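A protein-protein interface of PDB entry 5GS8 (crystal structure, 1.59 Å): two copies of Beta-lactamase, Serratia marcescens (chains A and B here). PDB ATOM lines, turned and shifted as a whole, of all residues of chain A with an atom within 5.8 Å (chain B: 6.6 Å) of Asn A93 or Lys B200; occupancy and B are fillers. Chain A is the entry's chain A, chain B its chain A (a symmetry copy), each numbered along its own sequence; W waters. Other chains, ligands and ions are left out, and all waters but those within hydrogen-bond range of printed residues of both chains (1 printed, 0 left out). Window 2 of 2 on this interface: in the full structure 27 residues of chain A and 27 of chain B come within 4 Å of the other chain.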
ATOM      1  N   LYS A  75      18.882  -9.627  18.120  1.00  0.00           N
ATOM      2  CA  LYS A  75      17.976  -8.486  17.939  1.00  0.00           C
ATOM      3  C   LYS A  75      18.519  -7.287  18.690  1.00  0.00           C
ATOM      4  O   LYS A  75      19.172  -7.428  19.708  1.00  0.00           O
ATOM      5  CB  LYS A  75      16.592  -8.839  18.507  1.00  0.00           C
ATOM      6  CG  LYS A  75      15.868  -9.879  17.667  1.00  0.00           C
ATOM      7  CD  LYS A  75      14.532 -10.277  18.277  1.00  0.00           C
ATOM      8  CE  LYS A  75      14.722 -11.272  19.397  1.00  0.00           C
ATOM      9  NZ  LYS A  75      14.050 -12.574  19.105  1.00  0.00           N
ATOM     10  N   LYS A  76      18.176  -6.068  18.276  1.00  0.00           N
ATOM     11  CA  LYS A  76      18.564  -4.911  19.069  1.00  0.00           C
ATOM     12  C   LYS A  76      17.985  -5.020  20.507  1.00  0.00           C
ATOM     13  O   LYS A  76      18.658  -4.655  21.478  1.00  0.00           O
ATOM     14  CB  LYS A  76      18.125  -3.626  18.364  1.00  0.00           C
ATOM     15  CG  LYS A  76      18.299  -2.352  19.191  1.00  0.00           C
ATOM     16  CD  LYS A  76      19.758  -1.990  19.363  1.00  0.00           C
ATOM     17  CE  LYS A  76      19.885  -0.582  19.974  1.00  0.00           C
ATOM     18  NZ  LYS A  76      18.833  -0.335  21.003  1.00  0.00           N
ATOM     19  N   LEU A  79      20.152  -6.563  23.113  1.00  0.00           N
ATOM     20  CA  LEU A  79      21.290  -5.739  23.583  1.00  0.00           C
ATOM     21  C   LEU A  79      20.751  -4.604  24.446  1.00  0.00           C
ATOM     22  O   LEU A  79      20.515  -3.457  23.969  1.00  0.00           O
ATOM     23  CB  LEU A  79      22.109  -5.227  22.395  1.00  0.00           C
ATOM     24  CG  LEU A  79      22.722  -6.331  21.520  1.00  0.00           C
ATOM     25  CD1 LEU A  79      23.481  -5.812  20.290  1.00  0.00           C
ATOM     26  CD2 LEU A  79      23.688  -7.195  22.321  1.00  0.00           C
ATOM     27  N   LYS A  88      27.352  -4.821  22.948  1.00  0.00           N
ATOM     28  CA  LYS A  88      26.478  -3.731  22.546  1.00  0.00           C
ATOM     29  C   LYS A  88      27.279  -2.529  22.067  1.00  0.00           C
ATOM     30  O   LYS A  88      26.913  -1.904  21.098  1.00  0.00           O
ATOM     31  CB  LYS A  88      25.504  -3.339  23.671  1.00  0.00           C
ATOM     32  CG  LYS A  88      24.593  -2.143  23.365  1.00  0.00           C
ATOM     33  CD  LYS A  88      23.770  -1.735  24.579  1.00  0.00           C
ATOM     34  CE  LYS A  88      23.205  -0.318  24.460  1.00  0.00           C
ATOM     35  NZ  LYS A  88      24.189   0.706  24.963  1.00  0.00           N
ATOM     36  N   TYR A  91      28.405  -3.417  18.537  1.00  0.00           N
ATOM     37  CA  TYR A  91      27.285  -3.492  17.588  1.00  0.00           C
ATOM     38  C   TYR A  91      26.070  -2.703  18.064  1.00  0.00           C
ATOM     39  O   TYR A  91      25.049  -3.258  18.437  1.00  0.00           O
ATOM     40  CB  TYR A  91      26.889  -4.967  17.393  1.00  0.00           C
ATOM     41  CG  TYR A  91      28.028  -5.880  16.946  1.00  0.00           C
ATOM     42  CD1 TYR A  91      28.608  -5.750  15.701  1.00  0.00           C
ATOM     43  CD2 TYR A  91      28.517  -6.855  17.772  1.00  0.00           C
ATOM     44  CE1 TYR A  91      29.671  -6.556  15.330  1.00  0.00           C
ATOM     45  CE2 TYR A  91      29.548  -7.688  17.404  1.00  0.00           C
ATOM     46  CZ  TYR A  91      30.105  -7.550  16.154  1.00  0.00           C
ATOM     47  OH  TYR A  91      31.074  -8.435  15.703  1.00  0.00           O
ATOM     48  N   PRO A  92      26.184  -1.384  18.130  1.00  0.00           N
ATOM     49  CA  PRO A  92      25.143  -0.589  18.734  1.00  0.00           C
ATOM     50  C   PRO A  92      23.783  -0.604  18.056  1.00  0.00           C
ATOM     51  O   PRO A  92      22.783  -0.339  18.735  1.00  0.00           O
ATOM     52  CB  PRO A  92      25.743   0.826  18.757  1.00  0.00           C
ATOM     53  CG  PRO A  92      26.804   0.798  17.731  1.00  0.00           C
ATOM     54  CD  PRO A  92      27.332  -0.590  17.687  1.00  0.00           C
ATOM     55  N   ASN A  93      23.709  -0.979  16.784  1.00  0.00           N
ATOM     56  CA  ASN A  93      22.426  -1.174  16.102  1.00  0.00           C
ATOM     57  C   ASN A  93      21.811  -2.541  16.314  1.00  0.00           C
ATOM     58  O   ASN A  93      20.613  -2.716  16.126  1.00  0.00           O
ATOM     59  CB  ASN A  93      22.565  -0.954  14.625  1.00  0.00           C
ATOM     60  CG  ASN A  93      22.480   0.489  14.247  1.00  0.00           C
ATOM     61  OD1 ASN A  93      21.365   1.016  14.130  1.00  0.00           O
ATOM     62  ND2 ASN A  93      23.584   1.187  14.370  1.00  0.00           N
ATOM     63  N   GLY A  94      22.584  -3.475  16.843  1.00  0.00           N
ATOM     64  CA  GLY A  94      22.169  -4.851  16.881  1.00  0.00           C
ATOM     65  C   GLY A  94      21.620  -5.308  15.543  1.00  0.00           C
ATOM     66  O   GLY A  94      22.088  -4.894  14.486  1.00  0.00           O
ATOM     67  N   ASN A  95      20.645  -6.199  15.636  1.00  0.00           N
ATOM     68  CA  ASN A  95      19.980  -6.789  14.462  1.00  0.00           C
ATOM     69  C   ASN A  95      20.981  -7.346  13.471  1.00  0.00           C
ATOM     70  O   ASN A  95      21.002  -7.001  12.285  1.00  0.00           O
ATOM     71  CB  ASN A  95      19.092  -5.757  13.810  1.00  0.00           C
ATOM     72  CG  ASN A  95      17.959  -5.332  14.707  1.00  0.00           C
ATOM     73  OD1 ASN A  95      17.427  -6.123  15.480  1.00  0.00           O
ATOM     74  ND2 ASN A  95      17.551  -4.073  14.576  1.00  0.00           N
ATOM     75  N   THR B 196      27.098   7.020  19.417  1.00  0.00           N
ATOM     76  CA  THR B 196      26.737   5.739  18.825  1.00  0.00           C
ATOM     77  C   THR B 196      25.577   5.035  19.506  1.00  0.00           C
ATOM     78  O   THR B 196      25.025   4.073  18.951  1.00  0.00           O
ATOM     79  CB  THR B 196      27.904   4.758  18.809  1.00  0.00           C
ATOM     80  OG1 THR B 196      28.380   4.549  20.123  1.00  0.00           O
ATOM     81  CG2 THR B 196      29.051   5.343  18.014  1.00  0.00           C
ATOM     82  N   THR B 197      25.210   5.471  20.702  1.00  0.00           N
ATOM     83  CA  THR B 197      24.070   4.897  21.384  1.00  0.00           C
ATOM     84  C   THR B 197      22.776   5.405  20.766  1.00  0.00           C
ATOM     85  O   THR B 197      22.746   6.366  19.981  1.00  0.00           O
ATOM     86  CB  THR B 197      24.103   5.207  22.883  1.00  0.00           C
ATOM     87  OG1 THR B 197      23.979   6.636  23.068  1.00  0.00           O
ATOM     88  CG2 THR B 197      25.407   4.729  23.505  1.00  0.00           C
ATOM     89  N   GLY B 198      21.711   4.679  21.042  1.00  0.00           N
ATOM     90  CA  GLY B 198      20.380   5.052  20.598  1.00  0.00           C
ATOM     91  C   GLY B 198      20.185   5.297  19.137  1.00  0.00           C
ATOM     92  O   GLY B 198      19.430   6.162  18.749  1.00  0.00           O
ATOM     93  N   PRO B 199      20.733   4.447  18.271  1.00  0.00           N
ATOM     94  CA  PRO B 199      20.531   4.697  16.830  1.00  0.00           C
ATOM     95  C   PRO B 199      19.087   4.533  16.357  1.00  0.00           C
ATOM     96  O   PRO B 199      18.745   5.029  15.277  1.00  0.00           O
ATOM     97  CB  PRO B 199      21.456   3.666  16.173  1.00  0.00           C
ATOM     98  CG  PRO B 199      21.524   2.556  17.180  1.00  0.00           C
ATOM     99  CD  PRO B 199      21.583   3.263  18.527  1.00  0.00           C
ATOM    100  N   LYS B 200      18.251   3.859  17.154  1.00  0.00           N
ATOM    101  CA  LYS B 200      16.830   3.721  16.818  1.00  0.00           C
ATOM    102  C   LYS B 200      15.931   4.585  17.651  1.00  0.00           C
ATOM    103  O   LYS B 200      14.731   4.348  17.664  1.00  0.00           O
ATOM    104  CB  LYS B 200      16.339   2.283  17.054  1.00  0.00           C
ATOM    105  CG  LYS B 200      17.296   1.204  16.589  1.00  0.00           C
ATOM    106  CD  LYS B 200      17.561   1.371  15.123  1.00  0.00           C
ATOM    107  CE  LYS B 200      17.779   0.009  14.455  1.00  0.00           C
ATOM    108  NZ  LYS B 200      18.805   0.127  13.397  1.00  0.00           N
ATOM    109  N   ARG B 201      16.476   5.652  18.235  1.00  0.00           N
ATOM    110  CA  ARG B 201      15.664   6.621  18.996  1.00  0.00           C
ATOM    111  C   ARG B 201      15.402   7.869  18.134  1.00  0.00           C
ATOM    112  O   ARG B 201      14.762   7.729  17.100  1.00  0.00           O
ATOM    113  CB  ARG B 201      16.304   6.888  20.357  1.00  0.00           C
ATOM    114  CG  ARG B 201      16.407   5.621  21.209  1.00  0.00           C
ATOM    115  CD  ARG B 201      16.937   5.873  22.605  1.00  0.00           C
ATOM    116  NE  ARG B 201      17.183   4.608  23.299  1.00  0.00           N
ATOM    117  CZ  ARG B 201      17.521   4.495  24.580  1.00  0.00           C
ATOM    118  NH1 ARG B 201      17.563   5.557  25.361  1.00  0.00           N
ATOM    119  NH2 ARG B 201      17.719   3.308  25.105  1.00  0.00           N
ATOM    120  N   LEU B 202      15.927   9.052  18.452  1.00  0.00           N
ATOM    121  CA  LEU B 202      15.640  10.214  17.595  1.00  0.00           C
ATOM    122  C   LEU B 202      15.967   9.969  16.147  1.00  0.00           C
ATOM    123  O   LEU B 202      15.205  10.395  15.282  1.00  0.00           O
ATOM    124  CB  LEU B 202      16.368  11.481  18.039  1.00  0.00           C
ATOM    125  CG  LEU B 202      15.927  12.040  19.397  1.00  0.00           C
ATOM    126  CD1 LEU B 202      16.875  13.117  19.889  1.00  0.00           C
ATOM    127  CD2 LEU B 202      14.502  12.577  19.355  1.00  0.00           C
ATOM    128  N   LYS B 203      17.102   9.321  15.878  1.00  0.00           N
ATOM    129  CA  LYS B 203      17.576   9.041  14.516  1.00  0.00           C
ATOM    130  C   LYS B 203      16.768   7.979  13.776  1.00  0.00           C
ATOM    131  O   LYS B 203      16.998   7.750  12.588  1.00  0.00           O
ATOM    132  CB  LYS B 203      19.027   8.564  14.551  1.00  0.00           C
ATOM    133  CG  LYS B 203      20.008   9.676  14.862  1.00  0.00           C
ATOM    134  CD  LYS B 203      21.348   9.102  15.277  1.00  0.00           C
ATOM    135  CE  LYS B 203      22.058   8.486  14.080  1.00  0.00           C
ATOM    136  NZ  LYS B 203      22.351   9.502  13.036  1.00  0.00           N
ATOM    137  N   GLY B 204      16.000   7.188  14.514  1.00  0.00           N
ATOM    138  CA  GLY B 204      15.549   5.886  14.018  1.00  0.00           C
ATOM    139  C   GLY B 204      14.796   5.879  12.700  1.00  0.00           C
ATOM    140  O   GLY B 204      14.974   4.968  11.891  1.00  0.00           O
ATOM    141  N   LEU B 205      13.942   6.860  12.487  1.00  0.00           N
ATOM    142  CA  LEU B 205      13.106   6.893  11.280  1.00  0.00           C
ATOM    143  C   LEU B 205      13.380   8.103  10.372  1.00  0.00           C
ATOM    144  O   LEU B 205      12.621   8.372   9.438  1.00  0.00           O
ATOM    145  CB  LEU B 205      11.613   6.812  11.679  1.00  0.00           C
ATOM    146  CG  LEU B 205      11.194   5.528  12.346  1.00  0.00           C
ATOM    147  CD1 LEU B 205       9.809   5.656  12.980  1.00  0.00           C
ATOM    148  CD2 LEU B 205      11.231   4.384  11.355  1.00  0.00           C
ATOM    149  N   ASP B 232      16.011  10.411  24.765  1.00  0.00           N
ATOM    150  CA  ASP B 232      16.999  10.865  23.777  1.00  0.00           C
ATOM    151  C   ASP B 232      16.753  12.362  23.571  1.00  0.00           C
ATOM    152  O   ASP B 232      15.590  12.789  23.443  1.00  0.00           O
ATOM    153  CB  ASP B 232      16.865  10.070  22.474  1.00  0.00           C
ATOM    154  CG  ASP B 232      18.090  10.160  21.558  1.00  0.00           C
ATOM    155  OD1 ASP B 232      19.179  10.557  22.046  1.00  0.00           O
ATOM    156  OD2 ASP B 232      17.992   9.730  20.388  1.00  0.00           O
ATOM    157  N   ASP B 258      11.598  -2.205  22.597  1.00  0.00           N
ATOM    158  CA  ASP B 258      11.376  -1.850  21.216  1.00  0.00           C
ATOM    159  C   ASP B 258      10.301  -0.775  21.079  1.00  0.00           C
ATOM    160  O   ASP B 258      10.444   0.152  20.296  1.00  0.00           O
ATOM    161  CB  ASP B 258      10.984  -3.074  20.401  1.00  0.00           C
ATOM    162  CG  ASP B 258       9.755  -3.760  20.943  1.00  0.00           C
ATOM    163  OD1 ASP B 258       9.705  -4.051  22.164  1.00  0.00           O
ATOM    164  OD2 ASP B 258       8.800  -3.942  20.167  1.00  0.00           O
ATOM    165  N   GLU B 261      11.697   2.720  22.426  1.00  0.00           N
ATOM    166  CA  GLU B 261      12.529   3.385  21.417  1.00  0.00           C
ATOM    167  C   GLU B 261      11.697   3.910  20.262  1.00  0.00           C
ATOM    168  O   GLU B 261      11.957   4.974  19.735  1.00  0.00           O
ATOM    169  CB  GLU B 261      13.634   2.472  20.907  1.00  0.00           C
ATOM    170  CG  GLU B 261      14.581   2.058  22.010  1.00  0.00           C
ATOM    171  CD  GLU B 261      15.908   1.561  21.483  1.00  0.00           C
ATOM    172  OE1 GLU B 261      15.962   0.448  20.954  1.00  0.00           O
ATOM    173  OE2 GLU B 261      16.933   2.220  21.737  1.00  0.00           O
ATOM    174  N   LYS B 262      10.746   3.113  19.794  1.00  0.00           N
ATOM    175  CA  LYS B 262       9.885   3.514  18.692  1.00  0.00           C
ATOM    176  C   LYS B 262       9.054   4.747  18.995  1.00  0.00           C
ATOM    177  O   LYS B 262       8.849   5.583  18.110  1.00  0.00           O
ATOM    178  CB  LYS B 262       8.969   2.343  18.311  1.00  0.00           C
ATOM    179  CG  LYS B 262       8.012   2.680  17.180  1.00  0.00           C
ATOM    180  CD  LYS B 262       8.692   2.535  15.870  1.00  0.00           C
ATOM    181  CE  LYS B 262       8.657   1.095  15.392  1.00  0.00           C
ATOM    182  NZ  LYS B 262       9.652   0.934  14.291  1.00  0.00           N
ATOM    183  N   ILE B 264      10.050   7.256  20.663  1.00  0.00           N
ATOM    184  CA  ILE B 264      10.950   8.392  20.387  1.00  0.00           C
ATOM    185  C   ILE B 264      11.104   8.617  18.881  1.00  0.00           C
ATOM    186  O   ILE B 264      10.988   9.742  18.384  1.00  0.00           O
ATOM    187  CB  ILE B 264      12.332   8.200  21.054  1.00  0.00           C
ATOM    188  CG1 ILE B 264      12.157   8.015  22.577  1.00  0.00           C
ATOM    189  CG2 ILE B 264      13.303   9.365  20.734  1.00  0.00           C
ATOM    190  CD1 ILE B 264      13.431   7.557  23.249  1.00  0.00           C
ATOM    191  N   ALA B 265      11.367   7.546  18.168  1.00  0.00           N
ATOM    192  CA  ALA B 265      11.622   7.621  16.753  1.00  0.00           C
ATOM    193  C   ALA B 265      10.423   8.192  16.018  1.00  0.00           C
ATOM    194  O   ALA B 265      10.571   8.987  15.097  1.00  0.00           O
ATOM    195  CB  ALA B 265      11.933   6.206  16.229  1.00  0.00           C
ATOM    196  N   GLU B 266       9.241   7.697  16.347  1.00  0.00           N
ATOM    197  CA  GLU B 266       8.011   8.119  15.642  1.00  0.00           C
ATOM    198  C   GLU B 266       7.683   9.566  15.927  1.00  0.00           C
ATOM    199  O   GLU B 266       7.289  10.314  15.030  1.00  0.00           O
ATOM    200  CB  GLU B 266       6.846   7.215  16.025  1.00  0.00           C
ATOM    201  CG  GLU B 266       6.992   5.800  15.483  1.00  0.00           C
ATOM    202  CD  GLU B 266       6.584   5.646  14.046  1.00  0.00           C
ATOM    203  OE1 GLU B 266       6.465   6.666  13.317  1.00  0.00           O
ATOM    204  OE2 GLU B 266       6.485   4.473  13.611  1.00  0.00           O
HETATM  205  O   HOH W   1      18.430   2.571  19.593  1.00  0.00           O
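The side-chain carboxylate of Glu B261 is in salt-bridge range of the side-chain amino group of Lys A76 (3.0 Å).
The side-chain amide oxygen (OD1) of Asn A93 sits at hydrogen-bond distance from the side-chain amino group (NZ) of Lys B200 (2.8 Å).
The side-chain amide oxygen (OD1) of Asn A95 is in hydrogen-bond range of the backbone NH (N) of Lys A76 (2.9 Å).
NE of Arg B201 is in salt-bridge range of OE2 of Glu B261 (2.9 Å).
Pro A92 touches Thr B196 (CB to O, 3.3 Å).
O of Pro A92 touches CG of Pro B199, 3.5 Å away.
Asn A93 touches Pro B199.
Asn A93 touches two residues of chain B.
Lys B200 touches just one residue of chain A: Asn A93.
Of the printed residues of chain B, Lys A76 touches Glu B261.
Printed residues of chain B within 4 Å of Pro A92: Thr B196 (3.3 Å) and Pro B199 (3.5 Å).
Printed residues of chain A within 4 Å of Pro B199: Pro A92 (3.5 Å) and Asn A93 (3.3 Å).
Printed residues of chain A within 4 Å of Glu B261: Lys A76.
Arg B201 touches none of the printed residues of chain A.
Ala B265 touches none of the printed residues of chain A.
Of the 9 printed residues of chain A, 3 touch a printed residue of chain B.
Hydrophobic or aromatic side chains of chain A that line the printed part of chain B: Pro A92.
Of the 17 printed residues of chain B, 4 touch a printed residue of chain A.
Printed residues of chain B that touch a printed residue of chain A: Thr B196, Pro B199, Lys B200 and Glu B261.
Hydrophobic or aromatic side chains of chain B within 4 Å of the printed part of chain A: Pro B199.
Among the printed residues, 5 pairs touch across the chains.
No position is printed for both chains.
Of the 5 pairs that touch across the chains among the printed residues, none has its exchanged pair printed and touching as well.
Water W1 lies within hydrogen-bond range of the side-chain carboxylate of Glu B261 (2.6 Å), the backbone NH of Lys B200 (2.8 Å) and the side-chain amino group of Lys A76 (3.3 Å).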
